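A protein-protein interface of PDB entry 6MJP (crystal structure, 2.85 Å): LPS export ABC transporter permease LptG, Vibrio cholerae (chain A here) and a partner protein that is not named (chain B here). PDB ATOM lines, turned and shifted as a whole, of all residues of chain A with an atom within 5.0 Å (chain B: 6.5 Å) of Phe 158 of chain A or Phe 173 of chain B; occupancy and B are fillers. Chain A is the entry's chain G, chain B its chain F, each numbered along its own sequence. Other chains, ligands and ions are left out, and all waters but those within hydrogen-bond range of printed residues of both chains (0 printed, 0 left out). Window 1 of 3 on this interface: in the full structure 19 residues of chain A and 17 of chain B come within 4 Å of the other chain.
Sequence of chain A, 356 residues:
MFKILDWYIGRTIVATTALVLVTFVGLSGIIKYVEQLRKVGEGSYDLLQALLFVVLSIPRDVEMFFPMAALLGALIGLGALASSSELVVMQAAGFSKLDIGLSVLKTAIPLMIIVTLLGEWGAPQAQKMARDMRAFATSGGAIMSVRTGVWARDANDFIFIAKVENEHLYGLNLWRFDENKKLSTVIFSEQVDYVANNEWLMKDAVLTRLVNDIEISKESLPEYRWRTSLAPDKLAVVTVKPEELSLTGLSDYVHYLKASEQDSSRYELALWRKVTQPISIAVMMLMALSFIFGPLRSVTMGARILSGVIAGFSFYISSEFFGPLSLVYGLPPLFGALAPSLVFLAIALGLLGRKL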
ATOM      1  N   TRP A 151      27.960 -21.031  13.232  1.00  0.00           N
ATOM      2  CA  TRP A 151      26.523 -21.172  13.051  1.00  0.00           C
ATOM      3  C   TRP A 151      26.039 -22.489  13.648  1.00  0.00           C
ATOM      4  O   TRP A 151      26.751 -23.494  13.630  1.00  0.00           O
ATOM      5  CB  TRP A 151      26.146 -21.134  11.571  1.00  0.00           C
ATOM      6  CG  TRP A 151      26.070 -19.778  10.992  1.00  0.00           C
ATOM      7  CD1 TRP A 151      27.032 -19.143  10.268  1.00  0.00           C
ATOM      8  CD2 TRP A 151      24.958 -18.875  11.071  1.00  0.00           C
ATOM      9  NE1 TRP A 151      26.592 -17.894   9.887  1.00  0.00           N
ATOM     10  CE2 TRP A 151      25.322 -17.704  10.369  1.00  0.00           C
ATOM     11  CE3 TRP A 151      23.692 -18.939  11.665  1.00  0.00           C
ATOM     12  CZ2 TRP A 151      24.466 -16.608  10.249  1.00  0.00           C
ATOM     13  CZ3 TRP A 151      22.844 -17.846  11.542  1.00  0.00           C
ATOM     14  CH2 TRP A 151      23.235 -16.698  10.841  1.00  0.00           C
ATOM     15  N   ALA A 152      24.809 -22.492  14.153  1.00  0.00           N
ATOM     16  CA  ALA A 152      24.242 -23.734  14.664  1.00  0.00           C
ATOM     17  C   ALA A 152      22.721 -23.674  14.568  1.00  0.00           C
ATOM     18  O   ALA A 152      22.133 -22.604  14.397  1.00  0.00           O
ATOM     19  CB  ALA A 152      24.691 -24.004  16.104  1.00  0.00           C
ATOM     20  N   ARG A 153      22.093 -24.849  14.663  1.00  0.00           N
ATOM     21  CA  ARG A 153      20.644 -24.956  14.664  1.00  0.00           C
ATOM     22  C   ARG A 153      20.207 -25.814  15.842  1.00  0.00           C
ATOM     23  O   ARG A 153      20.808 -26.855  16.108  1.00  0.00           O
ATOM     24  CB  ARG A 153      20.109 -25.555  13.348  1.00  0.00           C
ATOM     25  CG  ARG A 153      18.585 -25.410  13.230  1.00  0.00           C
ATOM     26  CD  ARG A 153      18.003 -25.909  11.926  1.00  0.00           C
ATOM     27  NE  ARG A 153      18.085 -27.358  11.816  1.00  0.00           N
ATOM     28  CZ  ARG A 153      17.450 -28.062  10.888  1.00  0.00           C
ATOM     29  NH1 ARG A 153      16.680 -27.439  10.003  1.00  0.00           N
ATOM     30  NH2 ARG A 153      17.579 -29.383  10.845  1.00  0.00           N
ATOM     31  N   ASP A 154      19.164 -25.380  16.548  1.00  0.00           N
ATOM     32  CA  ASP A 154      18.532 -26.200  17.583  1.00  0.00           C
ATOM     33  C   ASP A 154      17.025 -26.194  17.335  1.00  0.00           C
ATOM     34  O   ASP A 154      16.342 -25.226  17.684  1.00  0.00           O
ATOM     35  CB  ASP A 154      18.873 -25.690  18.975  1.00  0.00           C
ATOM     36  CG  ASP A 154      18.361 -26.603  20.074  1.00  0.00           C
ATOM     37  OD1 ASP A 154      18.012 -27.775  19.792  1.00  0.00           O
ATOM     38  OD2 ASP A 154      18.307 -26.137  21.230  1.00  0.00           O
ATOM     39  N   ASN A 156      13.823 -25.372  15.701  1.00  0.00           N
ATOM     40  CA  ASN A 156      13.485 -24.247  14.845  1.00  0.00           C
ATOM     41  C   ASN A 156      14.360 -23.020  15.099  1.00  0.00           C
ATOM     42  O   ASN A 156      14.129 -21.969  14.488  1.00  0.00           O
ATOM     43  CB  ASN A 156      12.003 -23.893  15.018  1.00  0.00           C
ATOM     44  CG  ASN A 156      11.085 -24.823  14.240  1.00  0.00           C
ATOM     45  OD1 ASN A 156      11.438 -25.288  13.157  1.00  0.00           O
ATOM     46  ND2 ASN A 156       9.901 -25.099  14.789  1.00  0.00           N
ATOM     47  N   ASP A 157      15.368 -23.124  15.960  1.00  0.00           N
ATOM     48  CA  ASP A 157      16.222 -21.995  16.302  1.00  0.00           C
ATOM     49  C   ASP A 157      17.500 -22.013  15.480  1.00  0.00           C
ATOM     50  O   ASP A 157      18.100 -23.071  15.267  1.00  0.00           O
ATOM     51  CB  ASP A 157      16.588 -22.008  17.784  1.00  0.00           C
ATOM     52  CG  ASP A 157      15.382 -22.045  18.677  1.00  0.00           C
ATOM     53  OD1 ASP A 157      14.257 -22.215  18.158  1.00  0.00           O
ATOM     54  OD2 ASP A 157      15.565 -21.904  19.904  1.00  0.00           O
ATOM     55  N   PHE A 158      17.927 -20.830  15.044  1.00  0.00           N
ATOM     56  CA  PHE A 158      19.178 -20.648  14.313  1.00  0.00           C
ATOM     57  C   PHE A 158      20.063 -19.706  15.111  1.00  0.00           C
ATOM     58  O   PHE A 158      19.659 -18.579  15.417  1.00  0.00           O
ATOM     59  CB  PHE A 158      18.928 -20.090  12.913  1.00  0.00           C
ATOM     60  CG  PHE A 158      18.105 -20.988  12.050  1.00  0.00           C
ATOM     61  CD1 PHE A 158      16.720 -21.011  12.164  1.00  0.00           C
ATOM     62  CD2 PHE A 158      18.710 -21.815  11.124  1.00  0.00           C
ATOM     63  CE1 PHE A 158      15.961 -21.841  11.367  1.00  0.00           C
ATOM     64  CE2 PHE A 158      17.956 -22.649  10.323  1.00  0.00           C
ATOM     65  CZ  PHE A 158      16.583 -22.664  10.442  1.00  0.00           C
ATOM     66  N   ILE A 159      21.261 -20.162  15.445  1.00  0.00           N
ATOM     67  CA  ILE A 159      22.152 -19.426  16.330  1.00  0.00           C
ATOM     68  C   ILE A 159      23.396 -19.046  15.544  1.00  0.00           C
ATOM     69  O   ILE A 159      23.846 -19.801  14.676  1.00  0.00           O
ATOM     70  CB  ILE A 159      22.514 -20.254  17.585  1.00  0.00           C
ATOM     71  CG1 ILE A 159      21.250 -20.748  18.297  1.00  0.00           C
ATOM     72  CG2 ILE A 159      23.360 -19.443  18.546  1.00  0.00           C
ATOM     73  CD1 ILE A 159      20.852 -22.160  17.936  1.00  0.00           C
ATOM     74  N   PHE A 160      23.929 -17.860  15.822  1.00  0.00           N
ATOM     75  CA  PHE A 160      25.206 -17.430  15.266  1.00  0.00           C
ATOM     76  C   PHE A 160      26.039 -16.812  16.378  1.00  0.00           C
ATOM     77  O   PHE A 160      25.609 -15.839  17.010  1.00  0.00           O
ATOM     78  CB  PHE A 160      25.020 -16.434  14.117  1.00  0.00           C
ATOM     79  CG  PHE A 160      26.305 -15.817  13.670  1.00  0.00           C
ATOM     80  CD1 PHE A 160      27.173 -16.515  12.842  1.00  0.00           C
ATOM     81  CD2 PHE A 160      26.681 -14.559  14.120  1.00  0.00           C
ATOM     82  CE1 PHE A 160      28.378 -15.961  12.450  1.00  0.00           C
ATOM     83  CE2 PHE A 160      27.891 -14.001  13.731  1.00  0.00           C
ATOM     84  CZ  PHE A 160      28.736 -14.701  12.894  1.00  0.00           C
ATOM     85  N   ASN A 173      23.802 -14.377  18.644  1.00  0.00           N
ATOM     86  CA  ASN A 173      22.558 -14.004  17.982  1.00  0.00           C
ATOM     87  C   ASN A 173      21.732 -15.267  17.784  1.00  0.00           C
ATOM     88  O   ASN A 173      22.289 -16.333  17.515  1.00  0.00           O
ATOM     89  CB  ASN A 173      22.807 -13.318  16.627  1.00  0.00           C
ATOM     90  CG  ASN A 173      23.688 -12.081  16.740  1.00  0.00           C
ATOM     91  OD1 ASN A 173      23.208 -10.952  16.637  1.00  0.00           O
ATOM     92  ND2 ASN A 173      24.987 -12.291  16.934  1.00  0.00           N
ATOM     93  N   LEU A 174      20.410 -15.155  17.933  1.00  0.00           N
ATOM     94  CA  LEU A 174      19.530 -16.319  17.860  1.00  0.00           C
ATOM     95  C   LEU A 174      18.203 -15.917  17.243  1.00  0.00           C
ATOM     96  O   LEU A 174      17.630 -14.896  17.627  1.00  0.00           O
ATOM     97  CB  LEU A 174      19.303 -16.924  19.253  1.00  0.00           C
ATOM     98  CG  LEU A 174      18.117 -17.870  19.462  1.00  0.00           C
ATOM     99  CD1 LEU A 174      18.210 -18.998  18.481  1.00  0.00           C
ATOM    100  CD2 LEU A 174      18.088 -18.432  20.875  1.00  0.00           C
ATOM    101  N   TRP A 175      17.712 -16.728  16.309  1.00  0.00           N
ATOM    102  CA  TRP A 175      16.438 -16.498  15.643  1.00  0.00           C
ATOM    103  C   TRP A 175      15.537 -17.709  15.843  1.00  0.00           C
ATOM    104  O   TRP A 175      15.953 -18.842  15.575  1.00  0.00           O
ATOM    105  CB  TRP A 175      16.644 -16.235  14.147  1.00  0.00           C
ATOM    106  CG  TRP A 175      17.461 -15.011  13.836  1.00  0.00           C
ATOM    107  CD1 TRP A 175      16.988 -13.774  13.513  1.00  0.00           C
ATOM    108  CD2 TRP A 175      18.889 -14.914  13.797  1.00  0.00           C
ATOM    109  NE1 TRP A 175      18.030 -12.911  13.283  1.00  0.00           N
ATOM    110  CE2 TRP A 175      19.209 -13.585  13.450  1.00  0.00           C
ATOM    111  CE3 TRP A 175      19.929 -15.819  14.025  1.00  0.00           C
ATOM    112  CZ2 TRP A 175      20.525 -13.140  13.327  1.00  0.00           C
ATOM    113  CZ3 TRP A 175      21.238 -15.374  13.903  1.00  0.00           C
ATOM    114  CH2 TRP A 175      21.521 -14.047  13.556  1.00  0.00           C
ATOM    115  N   PHE A 177      11.795 -19.603  14.929  1.00  0.00           N
ATOM    116  CA  PHE A 177      10.714 -19.660  13.954  1.00  0.00           C
ATOM    117  C   PHE A 177       9.604 -20.586  14.443  1.00  0.00           C
ATOM    118  O   PHE A 177       9.869 -21.609  15.083  1.00  0.00           O
ATOM    119  CB  PHE A 177      11.239 -20.107  12.588  1.00  0.00           C
ATOM    120  CG  PHE A 177      12.161 -19.108  11.945  1.00  0.00           C
ATOM    121  CD1 PHE A 177      13.496 -19.034  12.312  1.00  0.00           C
ATOM    122  CD2 PHE A 177      11.688 -18.228  10.986  1.00  0.00           C
ATOM    123  CE1 PHE A 177      14.345 -18.103  11.725  1.00  0.00           C
ATOM    124  CE2 PHE A 177      12.527 -17.299  10.397  1.00  0.00           C
ATOM    125  CZ  PHE A 177      13.858 -17.236  10.767  1.00  0.00           C
ATOM    126  N   PHE B 149      25.376 -25.246   7.057  1.00  0.00           N
ATOM    127  CA  PHE B 149      25.402 -23.841   6.656  1.00  0.00           C
ATOM    128  C   PHE B 149      26.385 -23.666   5.502  1.00  0.00           C
ATOM    129  O   PHE B 149      27.600 -23.766   5.688  1.00  0.00           O
ATOM    130  CB  PHE B 149      25.759 -22.948   7.846  1.00  0.00           C
ATOM    131  CG  PHE B 149      24.680 -22.878   8.909  1.00  0.00           C
ATOM    132  CD1 PHE B 149      24.622 -23.826   9.921  1.00  0.00           C
ATOM    133  CD2 PHE B 149      23.721 -21.865   8.896  1.00  0.00           C
ATOM    134  CE1 PHE B 149      23.629 -23.771  10.897  1.00  0.00           C
ATOM    135  CE2 PHE B 149      22.729 -21.809   9.871  1.00  0.00           C
ATOM    136  CZ  PHE B 149      22.686 -22.763  10.872  1.00  0.00           C
ATOM    137  N   VAL B 158      24.837 -16.623   3.849  1.00  0.00           N
ATOM    138  CA  VAL B 158      24.935 -17.980   4.375  1.00  0.00           C
ATOM    139  C   VAL B 158      23.606 -18.678   4.117  1.00  0.00           C
ATOM    140  O   VAL B 158      22.563 -18.249   4.624  1.00  0.00           O
ATOM    141  CB  VAL B 158      25.280 -17.984   5.873  1.00  0.00           C
ATOM    142  CG1 VAL B 158      25.282 -19.396   6.415  1.00  0.00           C
ATOM    143  CG2 VAL B 158      26.622 -17.315   6.108  1.00  0.00           C
ATOM    144  N   VAL B 159      23.638 -19.751   3.332  1.00  0.00           N
ATOM    145  CA  VAL B 159      22.436 -20.471   2.929  1.00  0.00           C
ATOM    146  C   VAL B 159      22.385 -21.802   3.666  1.00  0.00           C
ATOM    147  O   VAL B 159      23.409 -22.470   3.832  1.00  0.00           O
ATOM    148  CB  VAL B 159      22.397 -20.692   1.406  1.00  0.00           C
ATOM    149  CG1 VAL B 159      21.044 -21.237   0.984  1.00  0.00           C
ATOM    150  CG2 VAL B 159      22.707 -19.397   0.681  1.00  0.00           C
ATOM    151  N   PHE B 160      21.191 -22.183   4.106  1.00  0.00           N
ATOM    152  CA  PHE B 160      20.985 -23.440   4.817  1.00  0.00           C
ATOM    153  C   PHE B 160      19.698 -24.055   4.286  1.00  0.00           C
ATOM    154  O   PHE B 160      18.610 -23.510   4.500  1.00  0.00           O
ATOM    155  CB  PHE B 160      20.922 -23.217   6.330  1.00  0.00           C
ATOM    156  CG  PHE B 160      20.616 -24.463   7.120  1.00  0.00           C
ATOM    157  CD1 PHE B 160      21.636 -25.284   7.569  1.00  0.00           C
ATOM    158  CD2 PHE B 160      19.304 -24.810   7.416  1.00  0.00           C
ATOM    159  CE1 PHE B 160      21.354 -26.437   8.294  1.00  0.00           C
ATOM    160  CE2 PHE B 160      19.017 -25.959   8.137  1.00  0.00           C
ATOM    161  CZ  PHE B 160      20.046 -26.774   8.576  1.00  0.00           C
ATOM    162  N   ILE B 161      19.821 -25.177   3.585  1.00  0.00           N
ATOM    163  CA  ILE B 161      18.688 -25.873   2.987  1.00  0.00           C
ATOM    164  C   ILE B 161      18.462 -27.172   3.752  1.00  0.00           C
ATOM    165  O   ILE B 161      19.419 -27.798   4.221  1.00  0.00           O
ATOM    166  CB  ILE B 161      18.922 -26.142   1.488  1.00  0.00           C
ATOM    167  CG1 ILE B 161      19.390 -24.869   0.785  1.00  0.00           C
ATOM    168  CG2 ILE B 161      17.660 -26.662   0.821  1.00  0.00           C
ATOM    169  CD1 ILE B 161      20.867 -24.859   0.500  1.00  0.00           C
ATOM    170  N   ASP B 162      17.192 -27.562   3.894  1.00  0.00           N
ATOM    171  CA  ASP B 162      16.837 -28.799   4.584  1.00  0.00           C
ATOM    172  C   ASP B 162      16.912 -30.008   3.657  1.00  0.00           C
ATOM    173  O   ASP B 162      17.712 -30.921   3.882  1.00  0.00           O
ATOM    174  CB  ASP B 162      15.432 -28.695   5.183  1.00  0.00           C
ATOM    175  CG  ASP B 162      15.392 -27.854   6.434  1.00  0.00           C
ATOM    176  OD1 ASP B 162      16.431 -27.244   6.762  1.00  0.00           O
ATOM    177  OD2 ASP B 162      14.327 -27.806   7.087  1.00  0.00           O
ATOM    178  N   ASN B 171      12.629 -25.740   2.315  1.00  0.00           N
ATOM    179  CA  ASN B 171      12.684 -25.132   3.644  1.00  0.00           C
ATOM    180  C   ASN B 171      13.998 -24.360   3.817  1.00  0.00           C
ATOM    181  O   ASN B 171      14.833 -24.675   4.670  1.00  0.00           O
ATOM    182  CB  ASN B 171      12.503 -26.200   4.743  1.00  0.00           C
ATOM    183  CG  ASN B 171      11.942 -25.658   6.025  1.00  0.00           C
ATOM    184  OD1 ASN B 171      11.101 -24.759   6.011  1.00  0.00           O
ATOM    185  ND2 ASN B 171      12.406 -26.202   7.149  1.00  0.00           N
ATOM    186  N   VAL B 172      14.174 -23.346   2.961  1.00  0.00           N
ATOM    187  CA  VAL B 172      15.421 -22.591   2.864  1.00  0.00           C
ATOM    188  C   VAL B 172      15.512 -21.547   3.969  1.00  0.00           C
ATOM    189  O   VAL B 172      14.511 -20.965   4.398  1.00  0.00           O
ATOM    190  CB  VAL B 172      15.529 -21.927   1.478  1.00  0.00           C
ATOM    191  CG1 VAL B 172      16.883 -21.271   1.301  1.00  0.00           C
ATOM    192  CG2 VAL B 172      15.273 -22.941   0.387  1.00  0.00           C
ATOM    193  N   PHE B 173      16.743 -21.299   4.417  1.00  0.00           N
ATOM    194  CA  PHE B 173      17.077 -20.233   5.354  1.00  0.00           C
ATOM    195  C   PHE B 173      18.297 -19.496   4.821  1.00  0.00           C
ATOM    196  O   PHE B 173      19.354 -20.106   4.639  1.00  0.00           O
ATOM    197  CB  PHE B 173      17.366 -20.794   6.750  1.00  0.00           C
ATOM    198  CG  PHE B 173      18.093 -19.832   7.658  1.00  0.00           C
ATOM    199  CD1 PHE B 173      17.388 -18.913   8.421  1.00  0.00           C
ATOM    200  CD2 PHE B 173      19.477 -19.842   7.752  1.00  0.00           C
ATOM    201  CE1 PHE B 173      18.047 -18.022   9.254  1.00  0.00           C
ATOM    202  CE2 PHE B 173      20.142 -18.950   8.580  1.00  0.00           C
ATOM    203  CZ  PHE B 173      19.428 -18.044   9.334  1.00  0.00           C
ATOM    204  N   VAL B 174      18.167 -18.190   4.597  1.00  0.00           N
ATOM    205  CA  VAL B 174      19.256 -17.375   4.071  1.00  0.00           C
ATOM    206  C   VAL B 174      19.592 -16.283   5.080  1.00  0.00           C
ATOM    207  O   VAL B 174      18.709 -15.523   5.501  1.00  0.00           O
ATOM    208  CB  VAL B 174      18.898 -16.761   2.706  1.00  0.00           C
ATOM    209  CG1 VAL B 174      20.084 -15.996   2.148  1.00  0.00           C
ATOM    210  CG2 VAL B 174      18.476 -17.840   1.744  1.00  0.00           C
ATOM    211  N   ALA B 175      20.868 -16.200   5.456  1.00  0.00           N
ATOM    212  CA  ALA B 175      21.347 -15.242   6.442  1.00  0.00           C
ATOM    213  C   ALA B 175      22.382 -14.333   5.807  1.00  0.00           C
ATOM    214  O   ALA B 175      23.312 -14.809   5.151  1.00  0.00           O
ATOM    215  CB  ALA B 175      21.956 -15.947   7.656  1.00  0.00           C
ATOM    216  N   VAL B 187      17.676 -11.386   6.958  1.00  0.00           N
ATOM    217  CA  VAL B 187      17.510 -12.817   7.172  1.00  0.00           C
ATOM    218  C   VAL B 187      16.145 -13.170   6.600  1.00  0.00           C
ATOM    219  O   VAL B 187      15.133 -12.589   7.011  1.00  0.00           O
ATOM    220  CB  VAL B 187      17.589 -13.211   8.662  1.00  0.00           C
ATOM    221  CG1 VAL B 187      17.035 -14.610   8.872  1.00  0.00           C
ATOM    222  CG2 VAL B 187      19.012 -13.137   9.182  1.00  0.00           C
ATOM    223  N   MET B 188      16.108 -14.094   5.639  1.00  0.00           N
ATOM    224  CA  MET B 188      14.853 -14.512   5.030  1.00  0.00           C
ATOM    225  C   MET B 188      14.705 -16.020   5.126  1.00  0.00           C
ATOM    226  O   MET B 188      15.695 -16.753   5.086  1.00  0.00           O
ATOM    227  CB  MET B 188      14.753 -14.068   3.566  1.00  0.00           C
ATOM    228  CG  MET B 188      15.799 -14.628   2.638  1.00  0.00           C
ATOM    229  SD  MET B 188      15.944 -13.529   1.224  1.00  0.00           S
ATOM    230  CE  MET B 188      17.182 -12.382   1.835  1.00  0.00           C
ATOM    231  N   PHE B 189      13.455 -16.465   5.249  1.00  0.00           N
ATOM    232  CA  PHE B 189      13.102 -17.869   5.398  1.00  0.00           C
ATOM    233  C   PHE B 189      11.890 -18.164   4.532  1.00  0.00           C
ATOM    234  O   PHE B 189      10.866 -17.485   4.642  1.00  0.00           O
ATOM    235  CB  PHE B 189      12.787 -18.213   6.854  1.00  0.00           C
ATOM    236  CG  PHE B 189      12.689 -19.686   7.115  1.00  0.00           C
ATOM    237  CD1 PHE B 189      13.823 -20.415   7.412  1.00  0.00           C
ATOM    238  CD2 PHE B 189      11.470 -20.346   7.055  1.00  0.00           C
ATOM    239  CE1 PHE B 189      13.751 -21.769   7.649  1.00  0.00           C
ATOM    240  CE2 PHE B 189      11.395 -21.708   7.290  1.00  0.00           C
ATOM    241  CZ  PHE B 189      12.542 -22.416   7.590  1.00  0.00           C
ATOM    242  N   SER B 190      11.995 -19.187   3.688  1.00  0.00           N
ATOM    243  CA  SER B 190      10.895 -19.528   2.796  1.00  0.00           C
ATOM    244  C   SER B 190      10.546 -21.009   2.897  1.00  0.00           C
ATOM    245  O   SER B 190      11.024 -21.710   3.796  1.00  0.00           O
ATOM    246  CB  SER B 190      11.246 -19.152   1.358  1.00  0.00           C
ATOM    247  OG  SER B 190      12.274 -19.981   0.858  1.00  0.00           O
ATOM    248  N   LEU B 207      13.449 -17.786  -4.205  1.00  0.00           N
ATOM    249  CA  LEU B 207      12.751 -18.324  -3.042  1.00  0.00           C
ATOM    250  C   LEU B 207      11.241 -18.219  -3.233  1.00  0.00           C
ATOM    251  O   LEU B 207      10.745 -17.238  -3.792  1.00  0.00           O
ATOM    252  CB  LEU B 207      13.152 -17.588  -1.752  1.00  0.00           C
ATOM    253  CG  LEU B 207      14.551 -17.882  -1.204  1.00  0.00           C
ATOM    254  CD1 LEU B 207      14.711 -17.325   0.195  1.00  0.00           C
ATOM    255  CD2 LEU B 207      14.823 -19.374  -1.210  1.00  0.00           C
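Among the printed residues, pairs that only touch across the chains: Arg 153 of chain A with Phe 160 of chain B (3.3 Å), Trp 151 of chain A with Phe 149 of chain B (3.5 Å), Trp 151 of chain A with Ala 175 of chain B (3.5 Å), Ala 152 of chain A with Phe 149 of chain B (3.6 Å), Phe 177 of chain A with Phe 189 of chain B (3.7 Å), Trp 151 of chain A with Val 158 of chain B (3.8 Å), Phe 158 of chain A with Phe 160 of chain B (3.9 Å) and Phe 158 of chain A with Phe 173 of chain B (3.9 Å).
The side-chain carboxylate of Asp 162 of chain B lies within salt-bridge range of the guanidinium group of Arg 153 of chain A, at 3.3 Å.
Hydrophobic or aromatic side chains of chain A that line the printed part of chain B: Trp 151, Phe 158 and Phe 177. Hydrophobic or aromatic side chains of chain B within 4 Å of the printed part of chain A: Phe 149, Val 158, Phe 160, Phe 173, Ala 175 and Phe 189.
Of the printed residues of chain A, Phe 173 of chain B touches Phe 158 (3.9 Å). Of the printed residues of chain A, Ala 175 of chain B touches Trp 151 (3.5 Å). Of the printed residues of chain A, Val 158 of chain B touches Trp 151. Leu 174 of chain A touches none of the printed residues of chain B. Ile 159 of chain A touches none of the printed residues of chain B. The nearest residue of chain A that does not touch Phe 173 of chain B is Trp 151 of chain A (4.1 Å).
The backbone carbonyl oxygen of Ala 152 of chain A lies within hydrogen-bond range of the backbone NH of Ile 159 of chain A. O of Ala 175 of chain B is in hydrogen-bond range of N of Val 158 of chain B (2.7 Å). N of Phe 160 of chain B lies within hydrogen-bond range of O of Phe 173 of chain B, at 2.8 Å. O of Asn 156 of chain A is in hydrogen-bond range of N of Phe 177 of chain A (3.4 Å). OD2 of Asp 162 of chain B is in hydrogen-bond range of ND2 of Asn 171 of chain B, at 2.5 Å. N of Trp 175 of chain A is in hydrogen-bond range of O of Phe 158 of chain A (2.8 Å).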
